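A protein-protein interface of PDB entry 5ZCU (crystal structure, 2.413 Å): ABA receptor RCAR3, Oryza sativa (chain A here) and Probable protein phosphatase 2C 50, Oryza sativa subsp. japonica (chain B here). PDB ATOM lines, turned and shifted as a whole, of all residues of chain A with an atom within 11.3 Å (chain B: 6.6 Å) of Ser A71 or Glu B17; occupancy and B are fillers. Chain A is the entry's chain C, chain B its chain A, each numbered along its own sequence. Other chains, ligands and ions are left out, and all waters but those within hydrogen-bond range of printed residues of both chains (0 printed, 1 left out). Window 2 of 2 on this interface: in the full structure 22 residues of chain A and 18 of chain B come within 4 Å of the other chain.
Of the 20 printed residues of chain A, 5 touch a printed residue of chain B.
Printed residues of chain A that touch a printed residue of chain B: Pro A48, Phe A49, Lys A70, Ser A71 and Gly A72.
Of the 21 printed residues of chain B, 5 touch a printed residue of chain A.
Printed residues of chain B that touch a printed residue of chain A: Glu B17, His B63, Gly B64, Asn B141 and Leu B211.
Hydrophobic or aromatic side chains of chain B that line the printed part of chain A: His B63 and Leu B211.
Among the printed residues, 8 pairs touch across the chains.
OE2 of Glu B17 lies within hydrogen-bond range of N of Gly B65 (2.9 Å).
The backbone NH (N) of His B63 lies within hydrogen-bond range of the backbone carbonyl oxygen (O) of Gly B143.
The backbone carbonyl oxygen of Pro A48 sits at hydrogen-bond distance from the side-chain amino group of Lys A70, 2.9 Å away.
N of Glu B17 sits at hydrogen-bond distance from OD1 of Asn B312 (2.7 Å).
The backbone carbonyl oxygen of Phe A49 sits at hydrogen-bond distance from the backbone NH of Lys A70.
The backbone carbonyl oxygen (O) of Glu B17 lies within hydrogen-bond range of the backbone NH (N) of Gly B62, at 2.9 Å.
Of the printed residues of chain B, Phe A49 touches Asn B141 (3.8 Å).
Printed residues of chain B within 4 Å of Lys A70: Gly B64.
No residue of chain A comes within 4 Å of Met B16.
Of chain A, only Ser A71 comes within 4 Å of Glu B17.
No residue of chain A comes within 4 Å of Asp B18.
No residue of chain A comes within 4 Å of Asp B61.
No residue of chain A comes within 4 Å of Gly B62.
Of the printed residues of chain A, His B63 touches Ser A71 (3.5 Å) and Gly A72 (3.9 Å).
Gly B65 touches none of the printed residues of chain A.
No residue of chain A comes within 4 Å of Ala B66.
No residue of chain A comes within 4 Å of Ala B69.
Printed residues of chain A within 4 Å of Asn B141: Pro A48 (3.2 Å) and Phe A49 (3.8 Å).
The nearest residue of chain B that does not touch Ser A71 is Gly B65 (4.05 Å).
The nearest residue of chain A that does not touch Glu B17 is Lys A70 (5.5 Å).
Among the printed residues, pairs that only touch across the chains: Ser A71 with His B63 (3.5 Å), Lys A70 with Gly B64 (3.8 Å), Gly A72 with Leu B211 (3.8 Å), Phe A49 with Asn B141 (3.8 Å) and Gly A72 with His B63 (3.9 Å).
The backbone NH of Gly B64 is in hydrogen-bond range of the side-chain hydroxyl of Ser A71 (2.9 Å).
ND2 of Asn B141 sits at hydrogen-bond distance from O of Pro A48 (3.2 Å).
OE2 of Glu B17 sits close to OG of Ser A71 (3.4 Å).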
ATOM      1  N   LYS A  47      23.654 -11.321 -16.906  1.00  0.00           N
ATOM      2  CA  LYS A  47      24.058  -9.950 -17.182  1.00  0.00           C
ATOM      3  C   LYS A  47      24.259  -9.791 -18.679  1.00  0.00           C
ATOM      4  O   LYS A  47      25.241 -10.324 -19.221  1.00  0.00           O
ATOM      5  CB  LYS A  47      25.342  -9.596 -16.431  1.00  0.00           C
ATOM      6  CG  LYS A  47      25.246  -9.744 -14.923  1.00  0.00           C
ATOM      7  CD  LYS A  47      26.517  -9.255 -14.240  1.00  0.00           C
ATOM      8  CE  LYS A  47      26.473  -9.518 -12.745  1.00  0.00           C
ATOM      9  NZ  LYS A  47      27.501  -8.730 -12.011  1.00  0.00           N
ATOM     10  N   PRO A  48      23.376  -9.080 -19.387  1.00  0.00           N
ATOM     11  CA  PRO A  48      23.511  -8.992 -20.849  1.00  0.00           C
ATOM     12  C   PRO A  48      24.727  -8.206 -21.303  1.00  0.00           C
ATOM     13  O   PRO A  48      25.114  -8.324 -22.471  1.00  0.00           O
ATOM     14  CB  PRO A  48      22.210  -8.306 -21.285  1.00  0.00           C
ATOM     15  CG  PRO A  48      21.751  -7.553 -20.078  1.00  0.00           C
ATOM     16  CD  PRO A  48      22.206  -8.338 -18.884  1.00  0.00           C
ATOM     17  N   PHE A  49      25.338  -7.405 -20.429  1.00  0.00           N
ATOM     18  CA  PHE A  49      26.493  -6.604 -20.813  1.00  0.00           C
ATOM     19  C   PHE A  49      27.789  -7.399 -20.880  1.00  0.00           C
ATOM     20  O   PHE A  49      28.761  -6.909 -21.461  1.00  0.00           O
ATOM     21  CB  PHE A  49      26.678  -5.439 -19.837  1.00  0.00           C
ATOM     22  CG  PHE A  49      25.435  -4.627 -19.618  1.00  0.00           C
ATOM     23  CD1 PHE A  49      24.947  -3.799 -20.616  1.00  0.00           C
ATOM     24  CD2 PHE A  49      24.759  -4.683 -18.409  1.00  0.00           C
ATOM     25  CE1 PHE A  49      23.805  -3.050 -20.415  1.00  0.00           C
ATOM     26  CE2 PHE A  49      23.617  -3.936 -18.205  1.00  0.00           C
ATOM     27  CZ  PHE A  49      23.140  -3.117 -19.207  1.00  0.00           C
ATOM     28  N   VAL A  50      27.833  -8.603 -20.322  1.00  0.00           N
ATOM     29  CA  VAL A  50      29.074  -9.360 -20.216  1.00  0.00           C
ATOM     30  C   VAL A  50      29.238 -10.211 -21.467  1.00  0.00           C
ATOM     31  O   VAL A  50      28.339 -10.978 -21.831  1.00  0.00           O
ATOM     32  CB  VAL A  50      29.081 -10.231 -18.950  1.00  0.00           C
ATOM     33  CG1 VAL A  50      30.284 -11.168 -18.952  1.00  0.00           C
ATOM     34  CG2 VAL A  50      29.078  -9.356 -17.704  1.00  0.00           C
ATOM     35  N   SER A  51      30.388 -10.076 -22.132  1.00  0.00           N
ATOM     36  CA  SER A  51      30.702 -10.884 -23.300  1.00  0.00           C
ATOM     37  C   SER A  51      31.761 -11.947 -23.052  1.00  0.00           C
ATOM     38  O   SER A  51      31.912 -12.844 -23.887  1.00  0.00           O
ATOM     39  CB  SER A  51      31.180  -9.991 -24.454  1.00  0.00           C
ATOM     40  OG  SER A  51      32.543  -9.648 -24.290  1.00  0.00           O
ATOM     41  N   ARG A  52      32.469 -11.887 -21.929  1.00  0.00           N
ATOM     42  CA  ARG A  52      33.365 -12.956 -21.516  1.00  0.00           C
ATOM     43  C   ARG A  52      33.802 -12.678 -20.083  1.00  0.00           C
ATOM     44  O   ARG A  52      33.768 -11.537 -19.615  1.00  0.00           O
ATOM     45  CB  ARG A  52      34.581 -13.049 -22.453  1.00  0.00           C
ATOM     46  CG  ARG A  52      35.576 -14.162 -22.164  1.00  0.00           C
ATOM     47  CD  ARG A  52      37.004 -13.679 -22.387  1.00  0.00           C
ATOM     48  NE  ARG A  52      37.206 -13.157 -23.736  1.00  0.00           N
ATOM     49  CZ  ARG A  52      38.212 -12.364 -24.093  1.00  0.00           C
ATOM     50  NH1 ARG A  52      39.089 -11.951 -23.191  1.00  0.00           N
ATOM     51  NH2 ARG A  52      38.315 -11.945 -25.348  1.00  0.00           N
ATOM     52  N   VAL A  67      36.308  -9.559 -16.232  1.00  0.00           N
ATOM     53  CA  VAL A  67      35.068  -9.423 -16.986  1.00  0.00           C
ATOM     54  C   VAL A  67      35.322  -8.520 -18.181  1.00  0.00           C
ATOM     55  O   VAL A  67      35.883  -7.427 -18.035  1.00  0.00           O
ATOM     56  CB  VAL A  67      33.940  -8.863 -16.103  1.00  0.00           C
ATOM     57  CG1 VAL A  67      32.666  -8.681 -16.916  1.00  0.00           C
ATOM     58  CG2 VAL A  67      33.702  -9.774 -14.909  1.00  0.00           C
ATOM     59  N   ASN A  68      34.909  -8.975 -19.359  1.00  0.00           N
ATOM     60  CA  ASN A  68      34.916  -8.166 -20.570  1.00  0.00           C
ATOM     61  C   ASN A  68      33.477  -7.877 -20.969  1.00  0.00           C
ATOM     62  O   ASN A  68      32.666  -8.802 -21.092  1.00  0.00           O
ATOM     63  CB  ASN A  68      35.657  -8.880 -21.703  1.00  0.00           C
ATOM     64  CG  ASN A  68      37.157  -8.908 -21.491  1.00  0.00           C
ATOM     65  OD1 ASN A  68      37.868  -7.985 -21.887  1.00  0.00           O
ATOM     66  ND2 ASN A  68      37.646  -9.971 -20.864  1.00  0.00           N
ATOM     67  N   VAL A  69      33.163  -6.601 -21.171  1.00  0.00           N
ATOM     68  CA  VAL A  69      31.810  -6.188 -21.501  1.00  0.00           C
ATOM     69  C   VAL A  69      31.733  -5.851 -22.985  1.00  0.00           C
ATOM     70  O   VAL A  69      32.742  -5.607 -23.654  1.00  0.00           O
ATOM     71  CB  VAL A  69      31.339  -5.002 -20.629  1.00  0.00           C
ATOM     72  CG1 VAL A  69      31.295  -5.405 -19.161  1.00  0.00           C
ATOM     73  CG2 VAL A  69      32.240  -3.809 -20.828  1.00  0.00           C
ATOM     74  N   LYS A  70      30.508  -5.843 -23.510  1.00  0.00           N
ATOM     75  CA  LYS A  70      30.278  -5.684 -24.938  1.00  0.00           C
ATOM     76  C   LYS A  70      30.366  -4.215 -25.349  1.00  0.00           C
ATOM     77  O   LYS A  70      30.670  -3.328 -24.545  1.00  0.00           O
ATOM     78  CB  LYS A  70      28.921  -6.268 -25.320  1.00  0.00           C
ATOM     79  CG  LYS A  70      28.561  -7.547 -24.587  1.00  0.00           C
ATOM     80  CD  LYS A  70      27.227  -8.100 -25.053  1.00  0.00           C
ATOM     81  CE  LYS A  70      27.098  -9.576 -24.717  1.00  0.00           C
ATOM     82  NZ  LYS A  70      25.680 -10.023 -24.709  1.00  0.00           N
ATOM     83  N   SER A  71      30.101  -3.960 -26.629  1.00  0.00           N
ATOM     84  CA  SER A  71      30.140  -2.612 -27.173  1.00  0.00           C
ATOM     85  C   SER A  71      28.970  -1.780 -26.648  1.00  0.00           C
ATOM     86  O   SER A  71      27.999  -2.298 -26.090  1.00  0.00           O
ATOM     87  CB  SER A  71      30.119  -2.654 -28.701  1.00  0.00           C
ATOM     88  OG  SER A  71      29.091  -3.508 -29.173  1.00  0.00           O
ATOM     89  N   GLY A  72      29.076  -0.467 -26.836  1.00  0.00           N
ATOM     90  CA  GLY A  72      28.025   0.437 -26.417  1.00  0.00           C
ATOM     91  C   GLY A  72      28.044   0.804 -24.953  1.00  0.00           C
ATOM     92  O   GLY A  72      27.006   1.199 -24.412  1.00  0.00           O
ATOM     93  N   LEU A  73      29.187   0.683 -24.294  1.00  0.00           N
ATOM     94  CA  LEU A  73      29.322   0.931 -22.868  1.00  0.00           C
ATOM     95  C   LEU A  73      30.504   1.856 -22.616  1.00  0.00           C
ATOM     96  O   LEU A  73      31.380   2.002 -23.473  1.00  0.00           O
ATOM     97  CB  LEU A  73      29.506  -0.392 -22.110  1.00  0.00           C
ATOM     98  CG  LEU A  73      28.273  -1.299 -22.152  1.00  0.00           C
ATOM     99  CD1 LEU A  73      28.596  -2.686 -21.613  1.00  0.00           C
ATOM    100  CD2 LEU A  73      27.117  -0.673 -21.386  1.00  0.00           C
ATOM    101  N   PRO A  74      30.556   2.496 -21.442  1.00  0.00           N
ATOM    102  CA  PRO A  74      31.716   3.351 -21.135  1.00  0.00           C
ATOM    103  C   PRO A  74      32.978   2.574 -20.812  1.00  0.00           C
ATOM    104  O   PRO A  74      34.074   3.133 -20.934  1.00  0.00           O
ATOM    105  CB  PRO A  74      31.248   4.174 -19.925  1.00  0.00           C
ATOM    106  CG  PRO A  74      29.811   3.817 -19.698  1.00  0.00           C
ATOM    107  CD  PRO A  74      29.558   2.512 -20.361  1.00  0.00           C
ATOM    108  N   ALA A  75      32.866   1.312 -20.414  1.00  0.00           N
ATOM    109  CA  ALA A  75      34.011   0.501 -20.028  1.00  0.00           C
ATOM    110  C   ALA A  75      34.140  -0.697 -20.960  1.00  0.00           C
ATOM    111  O   ALA A  75      33.264  -0.974 -21.780  1.00  0.00           O
ATOM    112  CB  ALA A  75      33.886   0.027 -18.575  1.00  0.00           C
ATOM    113  N   THR A  76      35.260  -1.393 -20.833  1.00  0.00           N
ATOM    114  CA  THR A  76      35.523  -2.607 -21.598  1.00  0.00           C
ATOM    115  C   THR A  76      35.902  -3.783 -20.713  1.00  0.00           C
ATOM    116  O   THR A  76      35.535  -4.921 -21.021  1.00  0.00           O
ATOM    117  CB  THR A  76      36.646  -2.363 -22.619  1.00  0.00           C
ATOM    118  OG1 THR A  76      37.859  -2.039 -21.927  1.00  0.00           O
ATOM    119  CG2 THR A  76      36.280  -1.217 -23.555  1.00  0.00           C
ATOM    120  N   ARG A  77      36.609  -3.535 -19.615  1.00  0.00           N
ATOM    121  CA  ARG A  77      37.096  -4.593 -18.748  1.00  0.00           C
ATOM    122  C   ARG A  77      36.852  -4.203 -17.300  1.00  0.00           C
ATOM    123  O   ARG A  77      36.686  -3.027 -16.968  1.00  0.00           O
ATOM    124  CB  ARG A  77      38.587  -4.868 -18.977  1.00  0.00           C
ATOM    125  CG  ARG A  77      39.471  -3.689 -18.638  1.00  0.00           C
ATOM    126  CD  ARG A  77      40.914  -3.945 -19.023  1.00  0.00           C
ATOM    127  NE  ARG A  77      41.679  -2.705 -19.055  1.00  0.00           N
ATOM    128  CZ  ARG A  77      42.192  -2.119 -17.979  1.00  0.00           C
ATOM    129  NH1 ARG A  77      42.022  -2.665 -16.782  1.00  0.00           N
ATOM    130  NH2 ARG A  77      42.874  -0.989 -18.099  1.00  0.00           N
ATOM    131  N   ASP A 100      38.685  -0.175 -16.511  1.00  0.00           N
ATOM    132  CA  ASP A 100      38.560   1.173 -17.050  1.00  0.00           C
ATOM    133  C   ASP A 100      37.171   1.769 -16.837  1.00  0.00           C
ATOM    134  O   ASP A 100      36.771   2.668 -17.586  1.00  0.00           O
ATOM    135  CB  ASP A 100      38.904   1.177 -18.542  1.00  0.00           C
ATOM    136  CG  ASP A 100      38.138   0.124 -19.326  1.00  0.00           C
ATOM    137  OD1 ASP A 100      37.270  -0.555 -18.737  1.00  0.00           O
ATOM    138  OD2 ASP A 100      38.401  -0.022 -20.538  1.00  0.00           O
ATOM    139  N   LEU A 149      22.397   0.404 -14.585  1.00  0.00           N
ATOM    140  CA  LEU A 149      23.010  -0.859 -14.981  1.00  0.00           C
ATOM    141  C   LEU A 149      22.550  -2.001 -14.084  1.00  0.00           C
ATOM    142  O   LEU A 149      22.271  -3.105 -14.570  1.00  0.00           O
ATOM    143  CB  LEU A 149      24.532  -0.728 -14.958  1.00  0.00           C
ATOM    144  CG  LEU A 149      25.123   0.150 -16.065  1.00  0.00           C
ATOM    145  CD1 LEU A 149      26.598   0.416 -15.813  1.00  0.00           C
ATOM    146  CD2 LEU A 149      24.911  -0.502 -17.423  1.00  0.00           C
ATOM    147  N   CYS A 152      18.909  -2.986 -15.015  1.00  0.00           N
ATOM    148  CA  CYS A 152      18.869  -3.827 -16.206  1.00  0.00           C
ATOM    149  C   CYS A 152      19.337  -5.248 -15.913  1.00  0.00           C
ATOM    150  O   CYS A 152      18.813  -6.205 -16.498  1.00  0.00           O
ATOM    151  CB  CYS A 152      19.717  -3.206 -17.315  1.00  0.00           C
ATOM    152  SG  CYS A 152      19.868  -4.229 -18.801  1.00  0.00           S
ATOM    153  N   ARG B  10      36.061  -5.559 -39.574  1.00  0.00           N
ATOM    154  CA  ARG B  10      36.230  -5.545 -38.121  1.00  0.00           C
ATOM    155  C   ARG B  10      37.167  -4.434 -37.643  1.00  0.00           C
ATOM    156  O   ARG B  10      36.835  -3.698 -36.704  1.00  0.00           O
ATOM    157  CB  ARG B  10      36.747  -6.914 -37.609  1.00  0.00           C
ATOM    158  CG  ARG B  10      35.862  -8.173 -37.814  1.00  0.00           C
ATOM    159  CD  ARG B  10      35.789  -8.569 -39.280  1.00  0.00           C
ATOM    160  NE  ARG B  10      34.874  -9.674 -39.472  1.00  0.00           N
ATOM    161  CZ  ARG B  10      34.416 -10.063 -40.655  1.00  0.00           C
ATOM    162  NH1 ARG B  10      34.766  -9.411 -41.755  1.00  0.00           N
ATOM    163  NH2 ARG B  10      33.576 -11.086 -40.735  1.00  0.00           N
ATOM    164  N   GLU B  15      34.680  -8.178 -32.591  1.00  0.00           N
ATOM    165  CA  GLU B  15      33.578  -8.704 -33.376  1.00  0.00           C
ATOM    166  C   GLU B  15      33.068  -7.644 -34.342  1.00  0.00           C
ATOM    167  O   GLU B  15      33.236  -6.442 -34.122  1.00  0.00           O
ATOM    168  CB  GLU B  15      32.440  -9.189 -32.467  1.00  0.00           C
ATOM    169  CG  GLU B  15      32.939  -9.897 -31.216  1.00  0.00           C
ATOM    170  CD  GLU B  15      32.014  -9.724 -30.029  1.00  0.00           C
ATOM    171  OE1 GLU B  15      32.517  -9.456 -28.917  1.00  0.00           O
ATOM    172  OE2 GLU B  15      30.785  -9.858 -30.207  1.00  0.00           O
ATOM    173  N   MET B  16      32.447  -8.110 -35.425  1.00  0.00           N
ATOM    174  CA  MET B  16      31.896  -7.235 -36.454  1.00  0.00           C
ATOM    175  C   MET B  16      30.427  -6.986 -36.138  1.00  0.00           C
ATOM    176  O   MET B  16      29.612  -7.915 -36.173  1.00  0.00           O
ATOM    177  CB  MET B  16      32.064  -7.863 -37.835  1.00  0.00           C
ATOM    178  CG  MET B  16      31.568  -6.998 -38.981  1.00  0.00           C
ATOM    179  SD  MET B  16      32.157  -5.299 -38.878  1.00  0.00           S
ATOM    180  CE  MET B  16      31.851  -4.737 -40.553  1.00  0.00           C
ATOM    181  N   GLU B  17      30.088  -5.736 -35.827  1.00  0.00           N
ATOM    182  CA  GLU B  17      28.711  -5.358 -35.536  1.00  0.00           C
ATOM    183  C   GLU B  17      28.196  -4.269 -36.468  1.00  0.00           C
ATOM    184  O   GLU B  17      27.084  -3.766 -36.264  1.00  0.00           O
ATOM    185  CB  GLU B  17      28.583  -4.930 -34.072  1.00  0.00           C
ATOM    186  CG  GLU B  17      28.971  -6.036 -33.103  1.00  0.00           C
ATOM    187  CD  GLU B  17      28.977  -5.585 -31.658  1.00  0.00           C
ATOM    188  OE1 GLU B  17      29.178  -4.378 -31.408  1.00  0.00           O
ATOM    189  OE2 GLU B  17      28.785  -6.443 -30.768  1.00  0.00           O
ATOM    190  N   ASP B  18      28.971  -3.895 -37.479  1.00  0.00           N
ATOM    191  CA  ASP B  18      28.507  -2.988 -38.515  1.00  0.00           C
ATOM    192  C   ASP B  18      27.774  -3.772 -39.596  1.00  0.00           C
ATOM    193  O   ASP B  18      28.055  -4.948 -39.837  1.00  0.00           O
ATOM    194  CB  ASP B  18      29.675  -2.221 -39.132  1.00  0.00           C
ATOM    195  CG  ASP B  18      29.974  -0.927 -38.408  1.00  0.00           C
ATOM    196  OD1 ASP B  18      29.355  -0.673 -37.352  1.00  0.00           O
ATOM    197  OD2 ASP B  18      30.833  -0.160 -38.895  1.00  0.00           O
ATOM    198  N   ALA B  19      26.825  -3.106 -40.246  1.00  0.00           N
ATOM    199  CA  ALA B  19      26.129  -3.675 -41.389  1.00  0.00           C
ATOM    200  C   ALA B  19      25.831  -2.565 -42.385  1.00  0.00           C
ATOM    201  O   ALA B  19      25.839  -1.380 -42.044  1.00  0.00           O
ATOM    202  CB  ALA B  19      24.835  -4.389 -40.972  1.00  0.00           C
ATOM    203  N   PHE B  60      24.571   0.799 -40.755  1.00  0.00           N
ATOM    204  CA  PHE B  60      23.970   0.493 -39.458  1.00  0.00           C
ATOM    205  C   PHE B  60      25.061   0.043 -38.491  1.00  0.00           C
ATOM    206  O   PHE B  60      25.518  -1.102 -38.548  1.00  0.00           O
ATOM    207  CB  PHE B  60      22.879  -0.562 -39.615  1.00  0.00           C
ATOM    208  CG  PHE B  60      21.988  -0.328 -40.804  1.00  0.00           C
ATOM    209  CD1 PHE B  60      20.960   0.598 -40.741  1.00  0.00           C
ATOM    210  CD2 PHE B  60      22.193  -1.012 -41.991  1.00  0.00           C
ATOM    211  CE1 PHE B  60      20.144   0.825 -41.833  1.00  0.00           C
ATOM    212  CE2 PHE B  60      21.381  -0.786 -43.086  1.00  0.00           C
ATOM    213  CZ  PHE B  60      20.354   0.133 -43.007  1.00  0.00           C
ATOM    214  N   ASP B  61      25.473   0.949 -37.607  1.00  0.00           N
ATOM    215  CA  ASP B  61      26.481   0.662 -36.591  1.00  0.00           C
ATOM    216  C   ASP B  61      25.786   0.027 -35.393  1.00  0.00           C
ATOM    217  O   ASP B  61      25.098   0.715 -34.631  1.00  0.00           O
ATOM    218  CB  ASP B  61      27.216   1.941 -36.194  1.00  0.00           C
ATOM    219  CG  ASP B  61      28.399   1.689 -35.265  1.00  0.00           C
ATOM    220  OD1 ASP B  61      28.448   0.638 -34.591  1.00  0.00           O
ATOM    221  OD2 ASP B  61      29.293   2.561 -35.209  1.00  0.00           O
ATOM    222  N   GLY B  62      25.971  -1.279 -35.222  1.00  0.00           N
ATOM    223  CA  GLY B  62      25.376  -1.964 -34.095  1.00  0.00           C
ATOM    224  C   GLY B  62      26.216  -1.852 -32.836  1.00  0.00           C
ATOM    225  O   GLY B  62      27.428  -1.652 -32.879  1.00  0.00           O
ATOM    226  N   HIS B  63      25.542  -1.980 -31.694  1.00  0.00           N
ATOM    227  CA  HIS B  63      26.202  -2.043 -30.397  1.00  0.00           C
ATOM    228  C   HIS B  63      25.515  -3.096 -29.542  1.00  0.00           C
ATOM    229  O   HIS B  63      24.328  -3.386 -29.723  1.00  0.00           O
ATOM    230  CB  HIS B  63      26.198  -0.687 -29.677  1.00  0.00           C
ATOM    231  CG  HIS B  63      24.882   0.025 -29.729  1.00  0.00           C
ATOM    232  ND1 HIS B  63      24.568   0.938 -30.711  1.00  0.00           N
ATOM    233  CD2 HIS B  63      23.802  -0.037 -28.914  1.00  0.00           C
ATOM    234  CE1 HIS B  63      23.351   1.407 -30.503  1.00  0.00           C
ATOM    235  NE2 HIS B  63      22.863   0.831 -29.418  1.00  0.00           N
ATOM    236  N   GLY B  64      26.277  -3.673 -28.612  1.00  0.00           N
ATOM    237  CA  GLY B  64      25.781  -4.768 -27.806  1.00  0.00           C
ATOM    238  C   GLY B  64      25.623  -6.067 -28.559  1.00  0.00           C
ATOM    239  O   GLY B  64      25.063  -7.022 -28.013  1.00  0.00           O
ATOM    240  N   GLY B  65      26.075  -6.132 -29.805  1.00  0.00           N
ATOM    241  CA  GLY B  65      25.807  -7.299 -30.621  1.00  0.00           C
ATOM    242  C   GLY B  65      25.504  -6.855 -32.035  1.00  0.00           C
ATOM    243  O   GLY B  65      25.415  -5.652 -32.285  1.00  0.00           O
ATOM    244  N   ALA B  66      25.348  -7.776 -32.980  1.00  0.00           N
ATOM    245  CA  ALA B  66      25.147  -7.378 -34.368  1.00  0.00           C
ATOM    246  C   ALA B  66      23.767  -7.671 -34.912  1.00  0.00           C
ATOM    247  O   ALA B  66      23.463  -7.291 -36.061  1.00  0.00           O
ATOM    248  CB  ALA B  66      26.171  -8.080 -35.256  1.00  0.00           C
ATOM    249  N   GLU B  67      22.969  -8.390 -34.129  1.00  0.00           N
ATOM    250  CA  GLU B  67      21.631  -8.818 -34.529  1.00  0.00           C
ATOM    251  C   GLU B  67      20.651  -7.707 -34.880  1.00  0.00           C
ATOM    252  O   GLU B  67      19.750  -7.908 -35.695  1.00  0.00           O
ATOM    253  CB  GLU B  67      21.022  -9.717 -33.449  1.00  0.00           C
ATOM    254  CG  GLU B  67      21.557  -9.459 -32.050  1.00  0.00           C
ATOM    255  CD  GLU B  67      22.648 -10.433 -31.655  1.00  0.00           C
ATOM    256  OE1 GLU B  67      23.833 -10.141 -31.920  1.00  0.00           O
ATOM    257  OE2 GLU B  67      22.321 -11.492 -31.078  1.00  0.00           O
ATOM    258  N   ALA B  69      21.628  -4.499 -36.007  1.00  0.00           N
ATOM    259  CA  ALA B  69      22.113  -3.882 -37.242  1.00  0.00           C
ATOM    260  C   ALA B  69      21.789  -4.740 -38.457  1.00  0.00           C
ATOM    261  O   ALA B  69      21.387  -4.222 -39.507  1.00  0.00           O
ATOM    262  CB  ALA B  69      23.616  -3.623 -37.160  1.00  0.00           C
ATOM    263  N   ASN B  70      21.982  -6.058 -38.338  1.00  0.00           N
ATOM    264  CA  ASN B  70      21.644  -6.958 -39.437  1.00  0.00           C
ATOM    265  C   ASN B  70      20.154  -6.908 -39.753  1.00  0.00           C
ATOM    266  O   ASN B  70      19.753  -7.000 -40.920  1.00  0.00           O
ATOM    267  CB  ASN B  70      22.072  -8.388 -39.104  1.00  0.00           C
ATOM    268  CG  ASN B  70      23.572  -8.591 -39.229  1.00  0.00           C
ATOM    269  OD1 ASN B  70      24.253  -7.860 -39.946  1.00  0.00           O
ATOM    270  ND2 ASN B  70      24.092  -9.590 -38.526  1.00  0.00           N
ATOM    271  N   ASN B 141      19.879  -4.838 -24.432  1.00  0.00           N
ATOM    272  CA  ASN B 141      20.993  -3.911 -24.587  1.00  0.00           C
ATOM    273  C   ASN B 141      21.532  -3.837 -26.010  1.00  0.00           C
ATOM    274  O   ASN B 141      22.522  -3.135 -26.242  1.00  0.00           O
ATOM    275  CB  ASN B 141      22.130  -4.290 -23.633  1.00  0.00           C
ATOM    276  CG  ASN B 141      22.747  -5.633 -23.965  1.00  0.00           C
ATOM    277  OD1 ASN B 141      22.043  -6.591 -24.278  1.00  0.00           O
ATOM    278  ND2 ASN B 141      24.071  -5.709 -23.905  1.00  0.00           N
ATOM    279  N   GLY B 143      21.438  -2.664 -29.862  1.00  0.00           N
ATOM    280  CA  GLY B 143      20.873  -1.607 -30.673  1.00  0.00           C
ATOM    281  C   GLY B 143      21.745  -1.343 -31.881  1.00  0.00           C
ATOM    282  O   GLY B 143      22.747  -2.024 -32.111  1.00  0.00           O
ATOM    283  N   SER B 144      21.352  -0.338 -32.662  1.00  0.00           N
ATOM    284  CA  SER B 144      22.081   0.006 -33.874  1.00  0.00           C
ATOM    285  C   SER B 144      21.727   1.422 -34.302  1.00  0.00           C
ATOM    286  O   SER B 144      20.582   1.856 -34.145  1.00  0.00           O
ATOM    287  CB  SER B 144      21.772  -0.976 -35.010  1.00  0.00           C
ATOM    288  OG  SER B 144      22.397  -0.562 -36.214  1.00  0.00           O
ATOM    289  N   LEU B 211      24.938   5.085 -22.871  1.00  0.00           N
ATOM    290  CA  LEU B 211      24.932   5.054 -24.329  1.00  0.00           C
ATOM    291  C   LEU B 211      25.337   6.404 -24.898  1.00  0.00           C
ATOM    292  O   LEU B 211      24.750   7.434 -24.548  1.00  0.00           O
ATOM    293  CB  LEU B 211      23.556   4.661 -24.862  1.00  0.00           C
ATOM    294  CG  LEU B 211      23.538   4.253 -26.335  1.00  0.00           C
ATOM    295  CD1 LEU B 211      24.417   3.029 -26.560  1.00  0.00           C
ATOM    296  CD2 LEU B 211      22.110   3.989 -26.802  1.00  0.00           C
ATOM    297  N   ASN B 312      34.782  -0.931 -35.756  1.00  0.00           N
ATOM    298  CA  ASN B 312      34.314  -1.420 -37.046  1.00  0.00           C
ATOM    299  C   ASN B 312      34.264  -0.267 -38.040  1.00  0.00           C
ATOM    300  O   ASN B 312      33.945   0.870 -37.676  1.00  0.00           O
ATOM    301  CB  ASN B 312      32.926  -2.054 -36.908  1.00  0.00           C
ATOM    302  CG  ASN B 312      32.927  -3.305 -36.043  1.00  0.00           C
ATOM    303  OD1 ASN B 312      31.874  -3.758 -35.589  1.00  0.00           O
ATOM    304  ND2 ASN B 312      34.108  -3.872 -35.819  1.00  0.00           N
